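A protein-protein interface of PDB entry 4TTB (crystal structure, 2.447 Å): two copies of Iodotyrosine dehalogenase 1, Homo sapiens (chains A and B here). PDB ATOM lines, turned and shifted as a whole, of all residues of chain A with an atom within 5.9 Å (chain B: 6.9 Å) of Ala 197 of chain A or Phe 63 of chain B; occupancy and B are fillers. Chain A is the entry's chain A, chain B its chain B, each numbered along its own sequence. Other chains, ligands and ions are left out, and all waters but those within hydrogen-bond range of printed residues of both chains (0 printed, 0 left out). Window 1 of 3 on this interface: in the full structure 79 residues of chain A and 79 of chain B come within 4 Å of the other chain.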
ATOM      1  N   PHE A  63       2.442 -22.972  13.802  1.00  0.00           N
ATOM      2  CA  PHE A  63       2.623 -21.539  13.985  1.00  0.00           C
ATOM      3  C   PHE A  63       3.798 -21.248  14.921  1.00  0.00           C
ATOM      4  O   PHE A  63       4.518 -20.263  14.757  1.00  0.00           O
ATOM      5  CB  PHE A  63       1.336 -20.936  14.554  1.00  0.00           C
ATOM      6  CG  PHE A  63       1.249 -19.444  14.428  1.00  0.00           C
ATOM      7  CD1 PHE A  63       1.326 -18.639  15.545  1.00  0.00           C
ATOM      8  CD2 PHE A  63       1.076 -18.849  13.192  1.00  0.00           C
ATOM      9  CE1 PHE A  63       1.231 -17.266  15.440  1.00  0.00           C
ATOM     10  CE2 PHE A  63       0.989 -17.471  13.079  1.00  0.00           C
ATOM     11  CZ  PHE A  63       1.070 -16.680  14.204  1.00  0.00           C
ATOM     12  N   ASN A  88      -0.346  -5.494   2.949  1.00  0.00           N
ATOM     13  CA  ASN A  88      -1.043  -6.558   3.645  1.00  0.00           C
ATOM     14  C   ASN A  88      -0.513  -6.738   5.039  1.00  0.00           C
ATOM     15  O   ASN A  88      -1.251  -7.018   5.979  1.00  0.00           O
ATOM     16  CB  ASN A  88      -0.939  -7.854   2.865  1.00  0.00           C
ATOM     17  CG  ASN A  88      -1.886  -7.888   1.688  1.00  0.00           C
ATOM     18  OD1 ASN A  88      -2.838  -7.108   1.622  1.00  0.00           O
ATOM     19  ND2 ASN A  88      -1.634  -8.788   0.753  1.00  0.00           N
ATOM     20  N   VAL A  89       0.783  -6.551   5.171  1.00  0.00           N
ATOM     21  CA  VAL A  89       1.440  -6.712   6.448  1.00  0.00           C
ATOM     22  C   VAL A  89       1.037  -5.574   7.393  1.00  0.00           C
ATOM     23  O   VAL A  89       0.852  -5.757   8.599  1.00  0.00           O
ATOM     24  CB  VAL A  89       2.966  -6.794   6.213  1.00  0.00           C
ATOM     25  CG1 VAL A  89       3.725  -6.186   7.335  1.00  0.00           C
ATOM     26  CG2 VAL A  89       3.381  -8.234   5.972  1.00  0.00           C
ATOM     27  N   THR A  92      -2.528  -6.056   8.487  1.00  0.00           N
ATOM     28  CA  THR A  92      -2.567  -7.098   9.498  1.00  0.00           C
ATOM     29  C   THR A  92      -2.263  -6.519  10.856  1.00  0.00           C
ATOM     30  O   THR A  92      -2.954  -6.811  11.827  1.00  0.00           O
ATOM     31  CB  THR A  92      -1.581  -8.218   9.182  1.00  0.00           C
ATOM     32  OG1 THR A  92      -1.946  -8.818   7.941  1.00  0.00           O
ATOM     33  CG2 THR A  92      -1.621  -9.287  10.247  1.00  0.00           C
ATOM     34  N   ALA A  93      -1.237  -5.677  10.911  1.00  0.00           N
ATOM     35  CA  ALA A  93      -0.891  -4.977  12.137  1.00  0.00           C
ATOM     36  C   ALA A  93      -2.070  -4.129  12.634  1.00  0.00           C
ATOM     37  O   ALA A  93      -2.274  -3.966  13.839  1.00  0.00           O
ATOM     38  CB  ALA A  93       0.301  -4.097  11.904  1.00  0.00           C
ATOM     39  N   GLY A 192       4.090  -6.186  17.417  1.00  0.00           N
ATOM     40  CA  GLY A 192       4.241  -7.630  17.572  1.00  0.00           C
ATOM     41  C   GLY A 192       3.532  -8.398  16.470  1.00  0.00           C
ATOM     42  O   GLY A 192       4.083  -9.348  15.902  1.00  0.00           O
ATOM     43  N   ILE A 193       2.310  -7.968  16.142  1.00  0.00           N
ATOM     44  CA  ILE A 193       1.535  -8.568  15.053  1.00  0.00           C
ATOM     45  C   ILE A 193       2.176  -8.312  13.680  1.00  0.00           C
ATOM     46  O   ILE A 193       2.208  -9.185  12.815  1.00  0.00           O
ATOM     47  CB  ILE A 193       0.058  -8.075  15.077  1.00  0.00           C
ATOM     48  CG1 ILE A 193      -0.679  -8.673  16.270  1.00  0.00           C
ATOM     49  CG2 ILE A 193      -0.667  -8.455  13.812  1.00  0.00           C
ATOM     50  CD1 ILE A 193      -2.063  -8.158  16.424  1.00  0.00           C
ATOM     51  N   LEU A 194       2.671  -7.099  13.490  1.00  0.00           N
ATOM     52  CA  LEU A 194       3.490  -6.755  12.338  1.00  0.00           C
ATOM     53  C   LEU A 194       4.685  -7.715  12.155  1.00  0.00           C
ATOM     54  O   LEU A 194       4.930  -8.213  11.055  1.00  0.00           O
ATOM     55  CB  LEU A 194       3.988  -5.324  12.511  1.00  0.00           C
ATOM     56  CG  LEU A 194       4.946  -4.681  11.519  1.00  0.00           C
ATOM     57  CD1 LEU A 194       4.294  -4.632  10.201  1.00  0.00           C
ATOM     58  CD2 LEU A 194       5.252  -3.267  11.970  1.00  0.00           C
ATOM     59  N   LEU A 195       5.415  -7.992  13.230  1.00  0.00           N
ATOM     60  CA  LEU A 195       6.591  -8.873  13.127  1.00  0.00           C
ATOM     61  C   LEU A 195       6.184 -10.288  12.751  1.00  0.00           C
ATOM     62  O   LEU A 195       6.826 -10.932  11.925  1.00  0.00           O
ATOM     63  CB  LEU A 195       7.407  -8.882  14.421  1.00  0.00           C
ATOM     64  CG  LEU A 195       8.058  -7.552  14.808  1.00  0.00           C
ATOM     65  CD1 LEU A 195       8.446  -7.559  16.276  1.00  0.00           C
ATOM     66  CD2 LEU A 195       9.287  -7.269  13.965  1.00  0.00           C
ATOM     67  N   ALA A 196       5.103 -10.766  13.350  1.00  0.00           N
ATOM     68  CA  ALA A 196       4.537 -12.049  12.960  1.00  0.00           C
ATOM     69  C   ALA A 196       4.152 -12.030  11.485  1.00  0.00           C
ATOM     70  O   ALA A 196       4.333 -13.019  10.778  1.00  0.00           O
ATOM     71  CB  ALA A 196       3.321 -12.374  13.811  1.00  0.00           C
ATOM     72  N   ALA A 197       3.654 -10.892  11.016  1.00  0.00           N
ATOM     73  CA  ALA A 197       3.220 -10.791   9.633  1.00  0.00           C
ATOM     74  C   ALA A 197       4.412 -10.819   8.685  1.00  0.00           C
ATOM     75  O   ALA A 197       4.344 -11.443   7.630  1.00  0.00           O
ATOM     76  CB  ALA A 197       2.376  -9.538   9.419  1.00  0.00           C
ATOM     77  N   LEU A 198       5.491 -10.133   9.058  1.00  0.00           N
ATOM     78  CA  LEU A 198       6.735 -10.181   8.290  1.00  0.00           C
ATOM     79  C   LEU A 198       7.283 -11.612   8.199  1.00  0.00           C
ATOM     80  O   LEU A 198       7.571 -12.117   7.111  1.00  0.00           O
ATOM     81  CB  LEU A 198       7.779  -9.246   8.893  1.00  0.00           C
ATOM     82  CG  LEU A 198       7.411  -7.762   8.827  1.00  0.00           C
ATOM     83  CD1 LEU A 198       8.408  -6.924   9.597  1.00  0.00           C
ATOM     84  CD2 LEU A 198       7.348  -7.302   7.392  1.00  0.00           C
ATOM     85  N   GLN A 199       7.408 -12.270   9.341  1.00  0.00           N
ATOM     86  CA  GLN A 199       7.895 -13.640   9.346  1.00  0.00           C
ATOM     87  C   GLN A 199       7.075 -14.522   8.405  1.00  0.00           C
ATOM     88  O   GLN A 199       7.625 -15.138   7.495  1.00  0.00           O
ATOM     89  CB  GLN A 199       7.919 -14.200  10.771  1.00  0.00           C
ATOM     90  CG  GLN A 199       8.455 -15.619  10.882  1.00  0.00           C
ATOM     91  CD  GLN A 199       9.888 -15.822  10.313  1.00  0.00           C
ATOM     92  OE1 GLN A 199      10.622 -14.871  10.010  1.00  0.00           O
ATOM     93  NE2 GLN A 199      10.270 -17.080  10.176  1.00  0.00           N
ATOM     94  N   ASN A 200       5.756 -14.523   8.595  1.00  0.00           N
ATOM     95  CA  ASN A 200       4.840 -15.327   7.786  1.00  0.00           C
ATOM     96  C   ASN A 200       4.958 -15.042   6.292  1.00  0.00           C
ATOM     97  O   ASN A 200       4.871 -15.953   5.470  1.00  0.00           O
ATOM     98  CB  ASN A 200       3.397 -15.118   8.262  1.00  0.00           C
ATOM     99  CG  ASN A 200       2.387 -15.848   7.409  1.00  0.00           C
ATOM    100  OD1 ASN A 200       2.101 -17.031   7.624  1.00  0.00           O
ATOM    101  ND2 ASN A 200       1.837 -15.147   6.431  1.00  0.00           N
ATOM    102  N   ALA A 201       5.168 -13.778   5.946  1.00  0.00           N
ATOM    103  CA  ALA A 201       5.383 -13.375   4.556  1.00  0.00           C
ATOM    104  C   ALA A 201       6.810 -13.655   4.030  1.00  0.00           C
ATOM    105  O   ALA A 201       7.105 -13.402   2.855  1.00  0.00           O
ATOM    106  CB  ALA A 201       5.054 -11.912   4.386  1.00  0.00           C
ATOM    107  N   GLY A 202       7.698 -14.119   4.908  1.00  0.00           N
ATOM    108  CA  GLY A 202       9.066 -14.425   4.520  1.00  0.00           C
ATOM    109  C   GLY A 202       9.929 -13.199   4.285  1.00  0.00           C
ATOM    110  O   GLY A 202      10.780 -13.168   3.397  1.00  0.00           O
ATOM    111  N   VAL B  57       2.396 -12.909  -1.622  1.00  0.00           N
ATOM    112  CA  VAL B  57       1.170 -12.148  -1.719  1.00  0.00           C
ATOM    113  C   VAL B  57       0.034 -12.931  -1.094  1.00  0.00           C
ATOM    114  O   VAL B  57      -0.594 -12.470  -0.144  1.00  0.00           O
ATOM    115  CB  VAL B  57       0.803 -11.879  -3.174  1.00  0.00           C
ATOM    116  CG1 VAL B  57      -0.542 -11.209  -3.242  1.00  0.00           C
ATOM    117  CG2 VAL B  57       1.871 -11.023  -3.835  1.00  0.00           C
ATOM    118  N   LYS B  58      -0.188 -14.131  -1.617  1.00  0.00           N
ATOM    119  CA  LYS B  58      -1.238 -15.019  -1.135  1.00  0.00           C
ATOM    120  C   LYS B  58      -1.106 -15.309   0.358  1.00  0.00           C
ATOM    121  O   LYS B  58      -2.089 -15.292   1.093  1.00  0.00           O
ATOM    122  CB  LYS B  58      -1.228 -16.320  -1.940  1.00  0.00           C
ATOM    123  CG  LYS B  58      -2.046 -17.439  -1.331  1.00  0.00           C
ATOM    124  CD  LYS B  58      -1.838 -18.744  -2.082  1.00  0.00           C
ATOM    125  CE  LYS B  58      -2.637 -18.779  -3.369  1.00  0.00           C
ATOM    126  NZ  LYS B  58      -4.104 -18.838  -3.100  1.00  0.00           N
ATOM    127  N   ARG B  59       0.115 -15.562   0.810  1.00  0.00           N
ATOM    128  CA  ARG B  59       0.340 -15.851   2.219  1.00  0.00           C
ATOM    129  C   ARG B  59       0.053 -14.643   3.095  1.00  0.00           C
ATOM    130  O   ARG B  59      -0.497 -14.783   4.188  1.00  0.00           O
ATOM    131  CB  ARG B  59       1.775 -16.326   2.466  1.00  0.00           C
ATOM    132  CG  ARG B  59       2.020 -17.771   2.105  1.00  0.00           C
ATOM    133  CD  ARG B  59       3.498 -18.131   2.274  1.00  0.00           C
ATOM    134  NE  ARG B  59       3.940 -18.029   3.662  1.00  0.00           N
ATOM    135  CZ  ARG B  59       3.863 -19.022   4.543  1.00  0.00           C
ATOM    136  NH1 ARG B  59       3.361 -20.199   4.184  1.00  0.00           N
ATOM    137  NH2 ARG B  59       4.287 -18.841   5.784  1.00  0.00           N
ATOM    138  N   SER B  60       0.450 -13.464   2.626  1.00  0.00           N
ATOM    139  CA  SER B  60       0.248 -12.245   3.400  1.00  0.00           C
ATOM    140  C   SER B  60      -1.237 -11.889   3.466  1.00  0.00           C
ATOM    141  O   SER B  60      -1.709 -11.381   4.481  1.00  0.00           O
ATOM    142  CB  SER B  60       1.062 -11.079   2.838  1.00  0.00           C
ATOM    143  OG  SER B  60       0.700 -10.783   1.505  1.00  0.00           O
ATOM    144  N   GLN B  61      -1.963 -12.172   2.385  1.00  0.00           N
ATOM    145  CA  GLN B  61      -3.409 -11.947   2.329  1.00  0.00           C
ATOM    146  C   GLN B  61      -4.155 -12.851   3.289  1.00  0.00           C
ATOM    147  O   GLN B  61      -4.937 -12.383   4.114  1.00  0.00           O
ATOM    148  CB  GLN B  61      -3.933 -12.208   0.930  1.00  0.00           C
ATOM    149  CG  GLN B  61      -3.638 -11.111  -0.053  1.00  0.00           C
ATOM    150  CD  GLN B  61      -4.465 -11.254  -1.305  1.00  0.00           C
ATOM    151  OE1 GLN B  61      -5.558 -11.826  -1.272  1.00  0.00           O
ATOM    152  NE2 GLN B  61      -3.947 -10.745  -2.423  1.00  0.00           N
ATOM    153  N   GLU B  62      -3.914 -14.150   3.157  1.00  0.00           N
ATOM    154  CA  GLU B  62      -4.506 -15.141   4.037  1.00  0.00           C
ATOM    155  C   GLU B  62      -4.315 -14.809   5.506  1.00  0.00           C
ATOM    156  O   GLU B  62      -5.237 -14.954   6.302  1.00  0.00           O
ATOM    157  CB  GLU B  62      -3.922 -16.515   3.733  1.00  0.00           C
ATOM    158  CG  GLU B  62      -4.362 -17.051   2.383  1.00  0.00           C
ATOM    159  CD  GLU B  62      -3.670 -18.343   2.014  1.00  0.00           C
ATOM    160  OE1 GLU B  62      -2.842 -18.827   2.817  1.00  0.00           O
ATOM    161  OE2 GLU B  62      -3.953 -18.872   0.918  1.00  0.00           O
ATOM    162  N   PHE B  63      -3.124 -14.347   5.858  1.00  0.00           N
ATOM    163  CA  PHE B  63      -2.806 -14.016   7.246  1.00  0.00           C
ATOM    164  C   PHE B  63      -3.539 -12.765   7.699  1.00  0.00           C
ATOM    165  O   PHE B  63      -3.953 -12.658   8.850  1.00  0.00           O
ATOM    166  CB  PHE B  63      -1.293 -13.826   7.404  1.00  0.00           C
ATOM    167  CG  PHE B  63      -0.821 -13.830   8.826  1.00  0.00           C
ATOM    168  CD1 PHE B  63      -0.311 -12.684   9.402  1.00  0.00           C
ATOM    169  CD2 PHE B  63      -0.861 -14.988   9.581  1.00  0.00           C
ATOM    170  CE1 PHE B  63       0.141 -12.687  10.710  1.00  0.00           C
ATOM    171  CE2 PHE B  63      -0.415 -14.997  10.891  1.00  0.00           C
ATOM    172  CZ  PHE B  63       0.086 -13.848  11.453  1.00  0.00           C
ATOM    173  N   TYR B  64      -3.687 -11.805   6.796  1.00  0.00           N
ATOM    174  CA  TYR B  64      -4.466 -10.628   7.114  1.00  0.00           C
ATOM    175  C   TYR B  64      -5.939 -10.995   7.368  1.00  0.00           C
ATOM    176  O   TYR B  64      -6.554 -10.522   8.327  1.00  0.00           O
ATOM    177  CB  TYR B  64      -4.370  -9.576   6.010  1.00  0.00           C
ATOM    178  CG  TYR B  64      -5.539  -8.604   6.068  1.00  0.00           C
ATOM    179  CD1 TYR B  64      -5.656  -7.690   7.114  1.00  0.00           C
ATOM    180  CD2 TYR B  64      -6.537  -8.631   5.108  1.00  0.00           C
ATOM    181  CE1 TYR B  64      -6.726  -6.823   7.189  1.00  0.00           C
ATOM    182  CE2 TYR B  64      -7.624  -7.767   5.180  1.00  0.00           C
ATOM    183  CZ  TYR B  64      -7.709  -6.862   6.218  1.00  0.00           C
ATOM    184  OH  TYR B  64      -8.778  -5.994   6.298  1.00  0.00           O
ATOM    185  N   GLU B  65      -6.501 -11.837   6.506  1.00  0.00           N
ATOM    186  CA  GLU B  65      -7.896 -12.249   6.640  1.00  0.00           C
ATOM    187  C   GLU B  65      -8.130 -13.017   7.931  1.00  0.00           C
ATOM    188  O   GLU B  65      -9.169 -12.884   8.564  1.00  0.00           O
ATOM    189  CB  GLU B  65      -8.324 -13.095   5.438  1.00  0.00           C
ATOM    190  CG  GLU B  65      -8.493 -12.280   4.161  1.00  0.00           C
ATOM    191  CD  GLU B  65      -8.514 -13.142   2.908  1.00  0.00           C
ATOM    192  OE1 GLU B  65      -8.531 -14.388   3.040  1.00  0.00           O
ATOM    193  OE2 GLU B  65      -8.507 -12.575   1.793  1.00  0.00           O
ATOM    194  N   LEU B  66      -7.147 -13.823   8.314  1.00  0.00           N
ATOM    195  CA  LEU B  66      -7.235 -14.641   9.513  1.00  0.00           C
ATOM    196  C   LEU B  66      -7.290 -13.745  10.735  1.00  0.00           C
ATOM    197  O   LEU B  66      -8.126 -13.915  11.620  1.00  0.00           O
ATOM    198  CB  LEU B  66      -6.000 -15.534   9.604  1.00  0.00           C
ATOM    199  CG  LEU B  66      -5.781 -16.324  10.889  1.00  0.00           C
ATOM    200  CD1 LEU B  66      -6.629 -17.563  10.866  1.00  0.00           C
ATOM    201  CD2 LEU B  66      -4.340 -16.689  11.019  1.00  0.00           C
ATOM    202  N   LEU B  67      -6.383 -12.782  10.770  1.00  0.00           N
ATOM    203  CA  LEU B  67      -6.221 -11.943  11.929  1.00  0.00           C
ATOM    204  C   LEU B  67      -7.289 -10.875  11.968  1.00  0.00           C
ATOM    205  O   LEU B  67      -7.657 -10.408  13.045  1.00  0.00           O
ATOM    206  CB  LEU B  67      -4.833 -11.291  11.934  1.00  0.00           C
ATOM    207  CG  LEU B  67      -3.627 -12.135  12.334  1.00  0.00           C
ATOM    208  CD1 LEU B  67      -2.630 -11.251  13.023  1.00  0.00           C
ATOM    209  CD2 LEU B  67      -3.996 -13.271  13.252  1.00  0.00           C
ATOM    210  N   ASN B  68      -7.776 -10.476  10.798  1.00  0.00           N
ATOM    211  CA  ASN B  68      -8.846  -9.481  10.752  1.00  0.00           C
ATOM    212  C   ASN B  68     -10.113 -10.006  11.431  1.00  0.00           C
ATOM    213  O   ASN B  68     -10.901  -9.230  11.935  1.00  0.00           O
ATOM    214  CB  ASN B  68      -9.114  -9.007   9.326  1.00  0.00           C
ATOM    215  CG  ASN B  68     -10.152  -7.893   9.252  1.00  0.00           C
ATOM    216  OD1 ASN B  68      -9.931  -6.755   9.698  1.00  0.00           O
ATOM    217  ND2 ASN B  68     -11.290  -8.213   8.657  1.00  0.00           N
ATOM    218  N   ALA B 196      -2.108 -13.156  18.199  1.00  0.00           N
ATOM    219  CA  ALA B 196      -2.050 -13.792  16.889  1.00  0.00           C
ATOM    220  C   ALA B 196      -2.140 -15.309  17.012  1.00  0.00           C
ATOM    221  O   ALA B 196      -2.884 -15.966  16.271  1.00  0.00           O
ATOM    222  CB  ALA B 196      -0.770 -13.407  16.186  1.00  0.00           C
ATOM    223  N   ASN B 200      -4.946 -17.752  15.603  1.00  0.00           N
ATOM    224  CA  ASN B 200      -4.586 -18.863  14.732  1.00  0.00           C
ATOM    225  C   ASN B 200      -5.054 -20.224  15.246  1.00  0.00           C
ATOM    226  O   ASN B 200      -5.475 -21.074  14.452  1.00  0.00           O
ATOM    227  CB  ASN B 200      -3.077 -18.869  14.462  1.00  0.00           C
ATOM    228  CG  ASN B 200      -2.650 -20.042  13.630  1.00  0.00           C
ATOM    229  OD1 ASN B 200      -2.765 -20.018  12.403  1.00  0.00           O
ATOM    230  ND2 ASN B 200      -2.166 -21.099  14.293  1.00  0.00           N
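The side-chain amide nitrogen of Asn 88 of chain A is in hydrogen-bond range of the side-chain hydroxyl of Ser 60 of chain B (3.2 Å).
O of Asn 200 of chain A lies within hydrogen-bond range of NE of Arg 59 of chain B, 2.9 Å away.
O of Asn 88 of chain A sits at hydrogen-bond distance from OG1 of Thr 92 of chain A (2.8 Å).
The side-chain hydroxyl of Ser 60 of chain B is in hydrogen-bond range of the backbone carbonyl oxygen of Val 57 of chain B.
Phe 63 of chain A touches Phe 63 of chain B (CE2 to CE2, 3.6 Å).
ND2 of Asn 200 of chain B touches CB of Phe 63 of chain A (3.5 Å).
Asn 88 of chain A touches Val 57 of chain B (ND2 to O, 3.9 Å).
Asn 88 of chain A touches Gln 61 of chain B.
Thr 92 of chain A touches Phe 63 of chain B.
Thr 92 of chain A touches Tyr 64 of chain B (OG1 to CB, 3.2 Å).
Leu 67 of chain B touches Thr 92 of chain A (CD1 to CG2, 3.5 Å).
Ile 193 of chain A touches Leu 67 of chain B (CG2 to CD1, 3.5 Å).
Ala 197 of chain A touches Phe 63 of chain B (CA to CE1, 3.8 Å).
CB of Phe 63 of chain B touches ND2 of Asn 200 of chain A, at 3.5 Å.
Ala 197 of chain A touches just one residue of chain B: Phe 63 (3.8 Å).
Phe 63 of chain B touches four residues of chain A.
Of the printed residues of chain B, Phe 63 of chain A touches Phe 63 (3.6 Å) and Asn 200 (3.5 Å).
Of the printed residues of chain B, Ile 193 of chain A touches Leu 67.
Of the printed residues of chain A, Leu 67 of chain B touches Thr 92 and Ile 193.
The nearest residue of chain B that does not touch Ala 197 of chain A is Ser 60 of chain B (5.8 Å).
The nearest residue of chain A that does not touch Phe 63 of chain B is Ala 196 of chain A (4.1 Å).
The nearest printed residue of chain A that does not touch Tyr 64 of chain B is Asn 88 of chain A (4.03 Å).
Of the 14 printed residues of chain B, 8 touch a printed residue of chain A.
Printed residues of chain B that touch a printed residue of chain A: Val 57, Arg 59, Ser 60, Gln 61, Phe 63, Tyr 64, Leu 67 and Asn 200.
Hydrophobic or aromatic side chains of chain B that line the printed part of chain A: Phe 63, Tyr 64 and Leu 67.
Printed residues of chain A that touch a printed residue of chain B: Phe 63, Asn 88, Thr 92, Ile 193, Ala 197 and Asn 200.
Among the printed residues, 12 pairs touch across the chains.
Among the printed residues, no Asp or Glu carboxylate lies within 4 Å of a Lys or Arg side-chain nitrogen of the other chain.
Phe 63 of chain A touches its own counterpart, Phe 63 of chain B.
Phe 63 of chain A touches Asn 200 of chain B, and with the chains exchanged Asn 200 of chain A touches Phe 63 of chain B.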
